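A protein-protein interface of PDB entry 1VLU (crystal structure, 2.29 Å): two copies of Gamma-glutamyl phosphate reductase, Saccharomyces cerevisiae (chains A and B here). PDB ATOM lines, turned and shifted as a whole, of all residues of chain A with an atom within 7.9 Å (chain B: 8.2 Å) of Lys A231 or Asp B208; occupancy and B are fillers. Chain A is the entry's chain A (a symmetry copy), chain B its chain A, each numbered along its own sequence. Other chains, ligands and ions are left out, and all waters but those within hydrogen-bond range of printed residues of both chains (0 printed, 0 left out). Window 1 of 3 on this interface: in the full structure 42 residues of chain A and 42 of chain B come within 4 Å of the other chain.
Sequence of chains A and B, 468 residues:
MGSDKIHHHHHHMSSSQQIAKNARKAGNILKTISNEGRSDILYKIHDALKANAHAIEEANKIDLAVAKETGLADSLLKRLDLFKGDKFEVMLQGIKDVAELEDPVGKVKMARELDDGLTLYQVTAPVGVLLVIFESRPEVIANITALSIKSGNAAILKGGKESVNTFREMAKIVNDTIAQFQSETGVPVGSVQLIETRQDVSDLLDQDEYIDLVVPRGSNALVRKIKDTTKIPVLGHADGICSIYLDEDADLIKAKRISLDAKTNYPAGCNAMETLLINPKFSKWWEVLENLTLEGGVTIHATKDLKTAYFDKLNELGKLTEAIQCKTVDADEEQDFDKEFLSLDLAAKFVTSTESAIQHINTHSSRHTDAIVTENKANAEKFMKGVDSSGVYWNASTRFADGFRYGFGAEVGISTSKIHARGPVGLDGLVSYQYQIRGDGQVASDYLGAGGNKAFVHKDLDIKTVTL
Printed residues of chain B within 4 Å of Asp A208: Asp B208 and Lys B231.
Of the printed residues of chain B, Glu A209 touches Lys B231 (3.97 Å).
Lys A231 touches just these residues of chain B: Asp B208 (3.5 Å) and Glu B209 (3.97 Å).
Of the printed residues of chain A, Glu B209 touches Lys A231.
Printed residues of chain A within 4 Å of Lys B231: Asp A208 and Glu A209.
The nearest residue of chain A that does not touch Asp B208 is Asp A206 (5.3 Å).
The nearest printed residue of chain A that does not touch Glu B209 is Asp A206 (4.4 Å).
Among the printed residues, merely in contact across the chains: Asp A208 with Lys B231 (3.5 Å), Glu A209 with Lys B231 (3.97 Å), Lys A231 with Asp B208 (3.5 Å) and Lys A231 with Glu B209 (3.97 Å).
Asp A208 touches its own counterpart, Asp B208.
Asp A208 touches Lys B231, and with the chains exchanged Lys A231 touches Asp B208.
Glu A209 touches Lys B231, and with the chains exchanged Lys A231 touches Glu B209.
Positions printed for both chains: 205, 206, 207, 208, 209, 211, 212, 214, 230, 231, 232 and 233.
Among the printed residues, 5 pairs touch across the chains.
Among the printed residues, no Asp or Glu carboxylate lies within 4 Å of a Lys or Arg side-chain nitrogen of the other chain.
OD2 of Asp B208 lies close to OD2 of Asp A208, at 2.7 Å.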
ATOM      1  N   LEU A 205      -4.202  20.383  15.547  1.00  0.00           N
ATOM      2  CA  LEU A 205      -3.595  19.752  16.711  1.00  0.00           C
ATOM      3  C   LEU A 205      -4.573  19.464  17.863  1.00  0.00           C
ATOM      4  O   LEU A 205      -4.232  18.727  18.804  1.00  0.00           O
ATOM      5  CB  LEU A 205      -2.409  20.579  17.191  1.00  0.00           C
ATOM      6  CG  LEU A 205      -1.136  20.438  16.348  1.00  0.00           C
ATOM      7  CD1 LEU A 205      -0.109  21.509  16.692  1.00  0.00           C
ATOM      8  CD2 LEU A 205      -0.529  19.046  16.470  1.00  0.00           C
ATOM      9  N   ASP A 206      -5.782  20.028  17.774  1.00  0.00           N
ATOM     10  CA  ASP A 206      -6.857  19.765  18.729  1.00  0.00           C
ATOM     11  C   ASP A 206      -7.776  18.603  18.297  1.00  0.00           C
ATOM     12  O   ASP A 206      -8.681  18.212  19.046  1.00  0.00           O
ATOM     13  CB  ASP A 206      -7.712  21.034  18.931  1.00  0.00           C
ATOM     14  CG  ASP A 206      -6.916  22.213  19.502  1.00  0.00           C
ATOM     15  OD1 ASP A 206      -5.834  21.997  20.100  1.00  0.00           O
ATOM     16  OD2 ASP A 206      -7.388  23.367  19.354  1.00  0.00           O
ATOM     17  N   GLN A 207      -7.549  18.047  17.105  1.00  0.00           N
ATOM     18  CA  GLN A 207      -8.469  17.050  16.551  1.00  0.00           C
ATOM     19  C   GLN A 207      -8.117  15.631  16.939  1.00  0.00           C
ATOM     20  O   GLN A 207      -8.130  14.759  16.106  1.00  0.00           O
ATOM     21  CB  GLN A 207      -8.560  17.162  15.015  1.00  0.00           C
ATOM     22  CG  GLN A 207      -8.932  18.561  14.480  1.00  0.00           C
ATOM     23  CD  GLN A 207     -10.146  19.120  15.176  1.00  0.00           C
ATOM     24  OE1 GLN A 207     -11.146  18.417  15.345  1.00  0.00           O
ATOM     25  NE2 GLN A 207     -10.063  20.380  15.608  1.00  0.00           N
ATOM     26  N   ASP A 208      -7.846  15.387  18.211  1.00  0.00           N
ATOM     27  CA  ASP A 208      -7.440  14.061  18.638  1.00  0.00           C
ATOM     28  C   ASP A 208      -8.531  12.987  18.669  1.00  0.00           C
ATOM     29  O   ASP A 208      -8.222  11.817  18.913  1.00  0.00           O
ATOM     30  CB  ASP A 208      -6.678  14.122  19.952  1.00  0.00           C
ATOM     31  CG  ASP A 208      -7.571  14.348  21.139  1.00  0.00           C
ATOM     32  OD1 ASP A 208      -8.559  15.106  21.026  1.00  0.00           O
ATOM     33  OD2 ASP A 208      -7.258  13.761  22.196  1.00  0.00           O
ATOM     34  N   GLU A 209      -9.781  13.358  18.388  1.00  0.00           N
ATOM     35  CA  GLU A 209     -10.823  12.350  18.161  1.00  0.00           C
ATOM     36  C   GLU A 209     -10.690  11.719  16.787  1.00  0.00           C
ATOM     37  O   GLU A 209     -11.204  10.632  16.554  1.00  0.00           O
ATOM     38  CB  GLU A 209     -12.244  12.927  18.279  1.00  0.00           C
ATOM     39  CG  GLU A 209     -12.395  14.101  19.214  1.00  0.00           C
ATOM     40  CD  GLU A 209     -12.266  15.436  18.480  1.00  0.00           C
ATOM     41  OE1 GLU A 209     -13.222  15.805  17.756  1.00  0.00           O
ATOM     42  OE2 GLU A 209     -11.218  16.114  18.633  1.00  0.00           O
ATOM     43  N   ILE A 211      -7.524  12.297  14.706  1.00  0.00           N
ATOM     44  CA  ILE A 211      -6.120  12.149  14.316  1.00  0.00           C
ATOM     45  C   ILE A 211      -5.399  11.314  15.330  1.00  0.00           C
ATOM     46  O   ILE A 211      -5.473  11.593  16.530  1.00  0.00           O
ATOM     47  CB  ILE A 211      -5.399  13.510  14.099  1.00  0.00           C
ATOM     48  CG1 ILE A 211      -6.137  14.349  13.051  1.00  0.00           C
ATOM     49  CG2 ILE A 211      -3.909  13.312  13.707  1.00  0.00           C
ATOM     50  CD1 ILE A 211      -5.635  15.813  12.931  1.00  0.00           C
ATOM     51  N   ASP A 212      -4.713  10.281  14.838  1.00  0.00           N
ATOM     52  CA  ASP A 212      -4.053   9.291  15.671  1.00  0.00           C
ATOM     53  C   ASP A 212      -2.561   9.497  15.904  1.00  0.00           C
ATOM     54  O   ASP A 212      -2.020   8.982  16.879  1.00  0.00           O
ATOM     55  CB  ASP A 212      -4.301   7.885  15.089  1.00  0.00           C
ATOM     56  CG  ASP A 212      -5.778   7.619  14.839  1.00  0.00           C
ATOM     57  OD1 ASP A 212      -6.504   7.397  15.841  1.00  0.00           O
ATOM     58  OD2 ASP A 212      -6.227   7.673  13.661  1.00  0.00           O
ATOM     59  N   VAL A 214       0.903  12.379  15.134  1.00  0.00           N
ATOM     60  CA  VAL A 214       1.562  13.516  14.535  1.00  0.00           C
ATOM     61  C   VAL A 214       2.959  13.118  14.166  1.00  0.00           C
ATOM     62  O   VAL A 214       3.689  12.579  15.002  1.00  0.00           O
ATOM     63  CB  VAL A 214       1.700  14.727  15.493  1.00  0.00           C
ATOM     64  CG1 VAL A 214       2.258  15.914  14.722  1.00  0.00           C
ATOM     65  CG2 VAL A 214       0.384  15.079  16.116  1.00  0.00           C
ATOM     66  N   ILE A 226       4.729  21.611  19.050  1.00  0.00           N
ATOM     67  CA  ILE A 226       3.719  20.583  18.799  1.00  0.00           C
ATOM     68  C   ILE A 226       3.368  19.846  20.089  1.00  0.00           C
ATOM     69  O   ILE A 226       2.204  19.713  20.418  1.00  0.00           O
ATOM     70  CB  ILE A 226       4.170  19.568  17.692  1.00  0.00           C
ATOM     71  CG1 ILE A 226       4.144  20.223  16.306  1.00  0.00           C
ATOM     72  CG2 ILE A 226       3.287  18.289  17.690  1.00  0.00           C
ATOM     73  CD1 ILE A 226       5.053  19.531  15.280  1.00  0.00           C
ATOM     74  N   LYS A 227       4.371  19.368  20.817  1.00  0.00           N
ATOM     75  CA  LYS A 227       4.126  18.689  22.084  1.00  0.00           C
ATOM     76  C   LYS A 227       3.267  19.491  23.058  1.00  0.00           C
ATOM     77  O   LYS A 227       2.388  18.934  23.701  1.00  0.00           O
ATOM     78  CB  LYS A 227       5.446  18.269  22.736  1.00  0.00           C
ATOM     79  CG  LYS A 227       5.650  16.774  22.771  1.00  0.00           C
ATOM     80  CD  LYS A 227       4.691  16.192  23.806  1.00  0.00           C
ATOM     81  CE  LYS A 227       4.578  14.703  23.746  1.00  0.00           C
ATOM     82  NZ  LYS A 227       3.360  14.337  24.509  1.00  0.00           N
ATOM     83  N   ASP A 228       3.486  20.801  23.141  1.00  0.00           N
ATOM     84  CA  ASP A 228       2.726  21.637  24.070  1.00  0.00           C
ATOM     85  C   ASP A 228       1.328  22.044  23.592  1.00  0.00           C
ATOM     86  O   ASP A 228       0.534  22.590  24.367  1.00  0.00           O
ATOM     87  CB  ASP A 228       3.534  22.873  24.482  1.00  0.00           C
ATOM     88  CG  ASP A 228       4.433  22.614  25.685  1.00  0.00           C
ATOM     89  OD1 ASP A 228       4.471  21.468  26.190  1.00  0.00           O
ATOM     90  OD2 ASP A 228       5.101  23.567  26.129  1.00  0.00           O
ATOM     91  N   THR A 229       1.011  21.757  22.337  1.00  0.00           N
ATOM     92  CA  THR A 229      -0.264  22.189  21.777  1.00  0.00           C
ATOM     93  C   THR A 229      -1.148  21.032  21.340  1.00  0.00           C
ATOM     94  O   THR A 229      -2.090  21.226  20.555  1.00  0.00           O
ATOM     95  CB  THR A 229      -0.059  23.128  20.573  1.00  0.00           C
ATOM     96  OG1 THR A 229       1.136  23.887  20.753  1.00  0.00           O
ATOM     97  CG2 THR A 229      -1.245  24.090  20.432  1.00  0.00           C
ATOM     98  N   THR A 230      -0.854  19.833  21.823  1.00  0.00           N
ATOM     99  CA  THR A 230      -1.587  18.671  21.334  1.00  0.00           C
ATOM    100  C   THR A 230      -1.704  17.552  22.336  1.00  0.00           C
ATOM    101  O   THR A 230      -0.820  17.364  23.162  1.00  0.00           O
ATOM    102  CB  THR A 230      -0.997  18.107  19.994  1.00  0.00           C
ATOM    103  OG1 THR A 230      -2.016  17.369  19.318  1.00  0.00           O
ATOM    104  CG2 THR A 230       0.201  17.191  20.236  1.00  0.00           C
ATOM    105  N   LYS A 231      -2.802  16.802  22.231  1.00  0.00           N
ATOM    106  CA  LYS A 231      -2.978  15.539  22.968  1.00  0.00           C
ATOM    107  C   LYS A 231      -2.817  14.295  22.078  1.00  0.00           C
ATOM    108  O   LYS A 231      -2.784  13.183  22.585  1.00  0.00           O
ATOM    109  CB  LYS A 231      -4.351  15.508  23.640  1.00  0.00           C
ATOM    110  CG  LYS A 231      -4.537  16.566  24.713  1.00  0.00           C
ATOM    111  CD  LYS A 231      -3.810  16.176  25.993  1.00  0.00           C
ATOM    112  CE  LYS A 231      -4.430  14.953  26.629  1.00  0.00           C
ATOM    113  NZ  LYS A 231      -3.750  14.677  27.920  1.00  0.00           N
ATOM    114  N   ILE A 232      -2.743  14.499  20.758  1.00  0.00           N
ATOM    115  CA  ILE A 232      -2.432  13.453  19.779  1.00  0.00           C
ATOM    116  C   ILE A 232      -1.005  12.987  20.017  1.00  0.00           C
ATOM    117  O   ILE A 232      -0.113  13.826  20.132  1.00  0.00           O
ATOM    118  CB  ILE A 232      -2.523  14.029  18.341  1.00  0.00           C
ATOM    119  CG1 ILE A 232      -3.871  14.733  18.119  1.00  0.00           C
ATOM    120  CG2 ILE A 232      -2.297  12.950  17.288  1.00  0.00           C
ATOM    121  CD1 ILE A 232      -3.875  15.731  16.974  1.00  0.00           C
ATOM    122  N   PRO A 233      -0.772  11.658  20.123  1.00  0.00           N
ATOM    123  CA  PRO A 233       0.624  11.178  20.204  1.00  0.00           C
ATOM    124  C   PRO A 233       1.545  11.700  19.081  1.00  0.00           C
ATOM    125  O   PRO A 233       1.131  11.810  17.916  1.00  0.00           O
ATOM    126  CB  PRO A 233       0.507   9.647  20.111  1.00  0.00           C
ATOM    127  CG  PRO A 233      -0.950   9.312  20.160  1.00  0.00           C
ATOM    128  CD  PRO A 233      -1.766  10.569  20.229  1.00  0.00           C
ATOM    129  N   VAL A 234       2.791  12.001  19.453  1.00  0.00           N
ATOM    130  CA  VAL A 234       3.799  12.473  18.541  1.00  0.00           C
ATOM    131  C   VAL A 234       4.808  11.368  18.287  1.00  0.00           C
ATOM    132  O   VAL A 234       5.403  10.843  19.229  1.00  0.00           O
ATOM    133  CB  VAL A 234       4.514  13.714  19.091  1.00  0.00           C
ATOM    134  CG1 VAL A 234       5.520  14.222  18.080  1.00  0.00           C
ATOM    135  CG2 VAL A 234       3.498  14.830  19.422  1.00  0.00           C
ATOM    136  N   SER A 365       2.184  20.205  28.233  1.00  0.00           N
ATOM    137  CA  SER A 365       1.314  19.064  28.023  1.00  0.00           C
ATOM    138  C   SER A 365       1.880  17.886  28.799  1.00  0.00           C
ATOM    139  O   SER A 365       3.095  17.628  28.759  1.00  0.00           O
ATOM    140  CB  SER A 365       1.263  18.728  26.537  1.00  0.00           C
ATOM    141  OG  SER A 365      -0.074  18.622  26.085  1.00  0.00           O
ATOM    142  N   SER A 366       0.988  17.168  29.484  1.00  0.00           N
ATOM    143  CA  SER A 366       1.373  16.213  30.530  1.00  0.00           C
ATOM    144  C   SER A 366       2.146  14.975  30.052  1.00  0.00           C
ATOM    145  O   SER A 366       2.347  14.762  28.848  1.00  0.00           O
ATOM    146  CB  SER A 366       0.155  15.818  31.385  1.00  0.00           C
ATOM    147  OG  SER A 366      -0.676  14.878  30.716  1.00  0.00           O
ATOM    148  N   ARG A 367       2.539  14.164  31.036  1.00  0.00           N
ATOM    149  CA  ARG A 367       3.552  13.108  30.917  1.00  0.00           C
ATOM    150  C   ARG A 367       4.947  13.735  30.915  1.00  0.00           C
ATOM    151  O   ARG A 367       5.719  13.574  29.966  1.00  0.00           O
ATOM    152  CB  ARG A 367       3.333  12.199  29.696  1.00  0.00           C
ATOM    153  N   ALA B  20     -12.927  25.887  30.232  1.00  0.00           N
ATOM    154  CA  ALA B  20     -11.996  24.827  30.584  1.00  0.00           C
ATOM    155  C   ALA B  20     -10.623  25.352  31.029  1.00  0.00           C
ATOM    156  O   ALA B  20     -10.009  24.805  31.954  1.00  0.00           O
ATOM    157  CB  ALA B  20     -11.847  23.841  29.434  1.00  0.00           C
ATOM    158  N   ARG B  24      -8.694  25.042  34.756  1.00  0.00           N
ATOM    159  CA  ARG B  24      -7.330  24.595  34.940  1.00  0.00           C
ATOM    160  C   ARG B  24      -6.535  25.574  35.806  1.00  0.00           C
ATOM    161  O   ARG B  24      -5.770  25.159  36.689  1.00  0.00           O
ATOM    162  CB  ARG B  24      -6.628  24.356  33.595  1.00  0.00           C
ATOM    163  CG  ARG B  24      -5.394  23.457  33.753  1.00  0.00           C
ATOM    164  CD  ARG B  24      -4.700  23.134  32.432  1.00  0.00           C
ATOM    165  NE  ARG B  24      -3.549  22.255  32.662  1.00  0.00           N
ATOM    166  CZ  ARG B  24      -2.305  22.670  32.918  1.00  0.00           C
ATOM    167  NH1 ARG B  24      -2.017  23.972  32.966  1.00  0.00           N
ATOM    168  NH2 ARG B  24      -1.340  21.771  33.134  1.00  0.00           N
ATOM    169  N   ASP B 203     -19.117  21.399  23.101  1.00  0.00           N
ATOM    170  CA  ASP B 203     -17.699  21.697  22.874  1.00  0.00           C
ATOM    171  C   ASP B 203     -16.801  21.419  24.091  1.00  0.00           C
ATOM    172  O   ASP B 203     -15.597  21.224  23.919  1.00  0.00           O
ATOM    173  CB  ASP B 203     -17.516  23.156  22.435  1.00  0.00           C
ATOM    174  CG  ASP B 203     -17.428  23.319  20.929  1.00  0.00           C
ATOM    175  OD1 ASP B 203     -17.543  22.312  20.197  1.00  0.00           O
ATOM    176  OD2 ASP B 203     -17.241  24.471  20.473  1.00  0.00           O
ATOM    177  N   LEU B 204     -17.379  21.420  25.299  1.00  0.00           N
ATOM    178  CA  LEU B 204     -16.648  21.095  26.538  1.00  0.00           C
ATOM    179  C   LEU B 204     -16.056  19.696  26.556  1.00  0.00           C
ATOM    180  O   LEU B 204     -15.004  19.483  27.140  1.00  0.00           O
ATOM    181  CB  LEU B 204     -17.532  21.266  27.776  1.00  0.00           C
ATOM    182  CG  LEU B 204     -17.734  22.656  28.366  1.00  0.00           C
ATOM    183  CD1 LEU B 204     -18.825  22.638  29.450  1.00  0.00           C
ATOM    184  CD2 LEU B 204     -16.439  23.260  28.892  1.00  0.00           C
ATOM    185  N   LEU B 205     -16.751  18.744  25.938  1.00  0.00           N
ATOM    186  CA  LEU B 205     -16.268  17.379  25.775  1.00  0.00           C
ATOM    187  C   LEU B 205     -15.056  17.239  24.838  1.00  0.00           C
ATOM    188  O   LEU B 205     -14.413  16.175  24.801  1.00  0.00           O
ATOM    189  CB  LEU B 205     -17.410  16.473  25.336  1.00  0.00           C
ATOM    190  CG  LEU B 205     -18.392  16.080  26.446  1.00  0.00           C
ATOM    191  CD1 LEU B 205     -19.656  15.445  25.884  1.00  0.00           C
ATOM    192  CD2 LEU B 205     -17.742  15.170  27.479  1.00  0.00           C
ATOM    193  N   ASP B 206     -14.741  18.312  24.106  1.00  0.00           N
ATOM    194  CA  ASP B 206     -13.557  18.375  23.251  1.00  0.00           C
ATOM    195  C   ASP B 206     -12.326  18.965  23.970  1.00  0.00           C
ATOM    196  O   ASP B 206     -11.228  19.005  23.397  1.00  0.00           O
ATOM    197  CB  ASP B 206     -13.853  19.215  21.991  1.00  0.00           C
ATOM    198  CG  ASP B 206     -14.972  18.627  21.123  1.00  0.00           C
ATOM    199  OD1 ASP B 206     -15.274  17.414  21.243  1.00  0.00           O
ATOM    200  OD2 ASP B 206     -15.547  19.390  20.309  1.00  0.00           O
ATOM    201  N   GLN B 207     -12.495  19.416  25.215  1.00  0.00           N
ATOM    202  CA  GLN B 207     -11.422  20.133  25.910  1.00  0.00           C
ATOM    203  C   GLN B 207     -10.502  19.222  26.690  1.00  0.00           C
ATOM    204  O   GLN B 207     -10.173  19.518  27.813  1.00  0.00           O
ATOM    205  CB  GLN B 207     -11.988  21.225  26.842  1.00  0.00           C
ATOM    206  CG  GLN B 207     -12.934  22.238  26.166  1.00  0.00           C
ATOM    207  CD  GLN B 207     -12.336  22.806  24.904  1.00  0.00           C
ATOM    208  OE1 GLN B 207     -11.165  23.198  24.891  1.00  0.00           O
ATOM    209  NE2 GLN B 207     -13.122  22.833  23.826  1.00  0.00           N
ATOM    210  N   ASP B 208     -10.046  18.137  26.085  1.00  0.00           N
ATOM    211  CA  ASP B 208      -9.211  17.190  26.800  1.00  0.00           C
ATOM    212  C   ASP B 208      -7.772  17.626  27.089  1.00  0.00           C
ATOM    213  O   ASP B 208      -7.051  16.911  27.790  1.00  0.00           O
ATOM    214  CB  ASP B 208      -9.257  15.820  26.142  1.00  0.00           C
ATOM    215  CG  ASP B 208      -8.448  15.746  24.879  1.00  0.00           C
ATOM    216  OD1 ASP B 208      -8.414  16.735  24.115  1.00  0.00           O
ATOM    217  OD2 ASP B 208      -7.853  14.670  24.656  1.00  0.00           O
ATOM    218  N   GLU B 209      -7.364  18.797  26.596  1.00  0.00           N
ATOM    219  CA  GLU B 209      -6.093  19.386  27.033  1.00  0.00           C
ATOM    220  C   GLU B 209      -6.216  19.998  28.417  1.00  0.00           C
ATOM    221  O   GLU B 209      -5.216  20.196  29.095  1.00  0.00           O
ATOM    222  CB  GLU B 209      -5.584  20.478  26.077  1.00  0.00           C
ATOM    223  CG  GLU B 209      -5.987  20.320  24.632  1.00  0.00           C
ATOM    224  CD  GLU B 209      -7.267  21.092  24.310  1.00  0.00           C
ATOM    225  OE1 GLU B 209      -7.195  22.341  24.222  1.00  0.00           O
ATOM    226  OE2 GLU B 209      -8.335  20.451  24.138  1.00  0.00           O
ATOM    227  N   TYR B 210      -7.439  20.337  28.817  1.00  0.00           N
ATOM    228  CA  TYR B 210      -7.673  21.032  30.073  1.00  0.00           C
ATOM    229  C   TYR B 210      -8.479  20.205  31.065  1.00  0.00           C
ATOM    230  O   TYR B 210      -8.370  20.430  32.264  1.00  0.00           O
ATOM    231  CB  TYR B 210      -8.395  22.350  29.838  1.00  0.00           C
ATOM    232  CG  TYR B 210      -7.729  23.308  28.879  1.00  0.00           C
ATOM    233  CD1 TYR B 210      -6.499  23.896  29.181  1.00  0.00           C
ATOM    234  CD2 TYR B 210      -8.357  23.662  27.685  1.00  0.00           C
ATOM    235  CE1 TYR B 210      -5.885  24.796  28.288  1.00  0.00           C
ATOM    236  CE2 TYR B 210      -7.765  24.555  26.786  1.00  0.00           C
ATOM    237  CZ  TYR B 210      -6.531  25.120  27.089  1.00  0.00           C
ATOM    238  OH  TYR B 210      -5.965  26.007  26.195  1.00  0.00           O
ATOM    239  N   ILE B 211      -9.307  19.283  30.566  1.00  0.00           N
ATOM    240  CA  ILE B 211     -10.204  18.503  31.422  1.00  0.00           C
ATOM    241  C   ILE B 211      -9.700  17.096  31.533  1.00  0.00           C
ATOM    242  O   ILE B 211      -9.427  16.451  30.516  1.00  0.00           O
ATOM    243  CB  ILE B 211     -11.683  18.531  30.942  1.00  0.00           C
ATOM    244  CG1 ILE B 211     -12.191  19.972  30.846  1.00  0.00           C
ATOM    245  CG2 ILE B 211     -12.599  17.677  31.862  1.00  0.00           C
ATOM    246  CD1 ILE B 211     -13.574  20.121  30.157  1.00  0.00           C
ATOM    247  N   ASP B 212      -9.568  16.631  32.777  1.00  0.00           N
ATOM    248  CA  ASP B 212      -8.982  15.339  33.089  1.00  0.00           C
ATOM    249  C   ASP B 212      -9.963  14.197  33.325  1.00  0.00           C
ATOM    250  O   ASP B 212      -9.588  13.035  33.191  1.00  0.00           O
ATOM    251  CB  ASP B 212      -8.045  15.483  34.304  1.00  0.00           C
ATOM    252  CG  ASP B 212      -7.037  16.609  34.123  1.00  0.00           C
ATOM    253  OD1 ASP B 212      -6.080  16.406  33.333  1.00  0.00           O
ATOM    254  OD2 ASP B 212      -7.215  17.703  34.724  1.00  0.00           O
ATOM    255  N   LEU B 213     -11.198  14.497  33.705  1.00  0.00           N
ATOM    256  CA  LEU B 213     -12.156  13.445  34.005  1.00  0.00           C
ATOM    257  C   LEU B 213     -13.560  13.933  33.803  1.00  0.00           C
ATOM    258  O   LEU B 213     -13.881  15.041  34.204  1.00  0.00           O
ATOM    259  CB  LEU B 213     -12.003  12.970  35.455  1.00  0.00           C
ATOM    260  CG  LEU B 213     -12.698  11.678  35.900  1.00  0.00           C
ATOM    261  CD1 LEU B 213     -12.177  10.455  35.137  1.00  0.00           C
ATOM    262  CD2 LEU B 213     -12.502  11.459  37.400  1.00  0.00           C
ATOM    263  N   VAL B 214     -14.397  13.090  33.204  1.00  0.00           N
ATOM    264  CA  VAL B 214     -15.815  13.345  33.106  1.00  0.00           C
ATOM    265  C   VAL B 214     -16.525  12.483  34.106  1.00  0.00           C
ATOM    266  O   VAL B 214     -16.298  11.271  34.149  1.00  0.00           O
ATOM    267  CB  VAL B 214     -16.415  12.978  31.724  1.00  0.00           C
ATOM    268  CG1 VAL B 214     -17.866  13.429  31.673  1.00  0.00           C
ATOM    269  CG2 VAL B 214     -15.633  13.605  30.610  1.00  0.00           C
ATOM    270  N   THR B 230     -16.203  12.162  23.242  1.00  0.00           N
ATOM    271  CA  THR B 230     -15.106  12.657  24.064  1.00  0.00           C
ATOM    272  C   THR B 230     -13.891  11.766  24.071  1.00  0.00           C
ATOM    273  O   THR B 230     -14.011  10.554  23.948  1.00  0.00           O
ATOM    274  CB  THR B 230     -15.546  12.945  25.543  1.00  0.00           C
ATOM    275  OG1 THR B 230     -14.638  13.887  26.117  1.00  0.00           O
ATOM    276  CG2 THR B 230     -15.552  11.679  26.396  1.00  0.00           C
ATOM    277  N   LYS B 231     -12.725  12.391  24.239  1.00  0.00           N
ATOM    278  CA  LYS B 231     -11.466  11.671  24.497  1.00  0.00           C
ATOM    279  C   LYS B 231     -11.003  11.772  25.961  1.00  0.00           C
ATOM    280  O   LYS B 231     -10.060  11.098  26.350  1.00  0.00           O
ATOM    281  CB  LYS B 231     -10.362  12.194  23.578  1.00  0.00           C
ATOM    282  CG  LYS B 231     -10.614  11.938  22.103  1.00  0.00           C
ATOM    283  CD  LYS B 231     -10.333  10.484  21.748  1.00  0.00           C
ATOM    284  CE  LYS B 231      -8.865  10.154  21.892  1.00  0.00           C
ATOM    285  NZ  LYS B 231      -8.632   8.759  21.439  1.00  0.00           N
ATOM    286  N   ILE B 232     -11.659  12.635  26.746  1.00  0.00           N
ATOM    287  CA  ILE B 232     -11.459  12.746  28.194  1.00  0.00           C
ATOM    288  C   ILE B 232     -11.925  11.451  28.839  1.00  0.00           C
ATOM    289  O   ILE B 232     -13.024  10.991  28.534  1.00  0.00           O
ATOM    290  CB  ILE B 232     -12.318  13.907  28.759  1.00  0.00           C
ATOM    291  CG1 ILE B 232     -12.063  15.205  27.977  1.00  0.00           C
ATOM    292  CG2 ILE B 232     -12.069  14.117  30.249  1.00  0.00           C
ATOM    293  CD1 ILE B 232     -13.169  16.239  28.102  1.00  0.00           C
ATOM    294  N   PRO B 233     -11.094  10.832  29.711  1.00  0.00           N
ATOM    295  CA  PRO B 233     -11.586   9.657  30.461  1.00  0.00           C
ATOM    296  C   PRO B 233     -12.917   9.885  31.206  1.00  0.00           C
ATOM    297  O   PRO B 233     -13.152  10.964  31.775  1.00  0.00           O
ATOM    298  CB  PRO B 233     -10.468   9.355  31.473  1.00  0.00           C
ATOM    299  CG  PRO B 233      -9.318  10.253  31.142  1.00  0.00           C
ATOM    300  CD  PRO B 233      -9.678  11.148  29.993  1.00  0.00           C
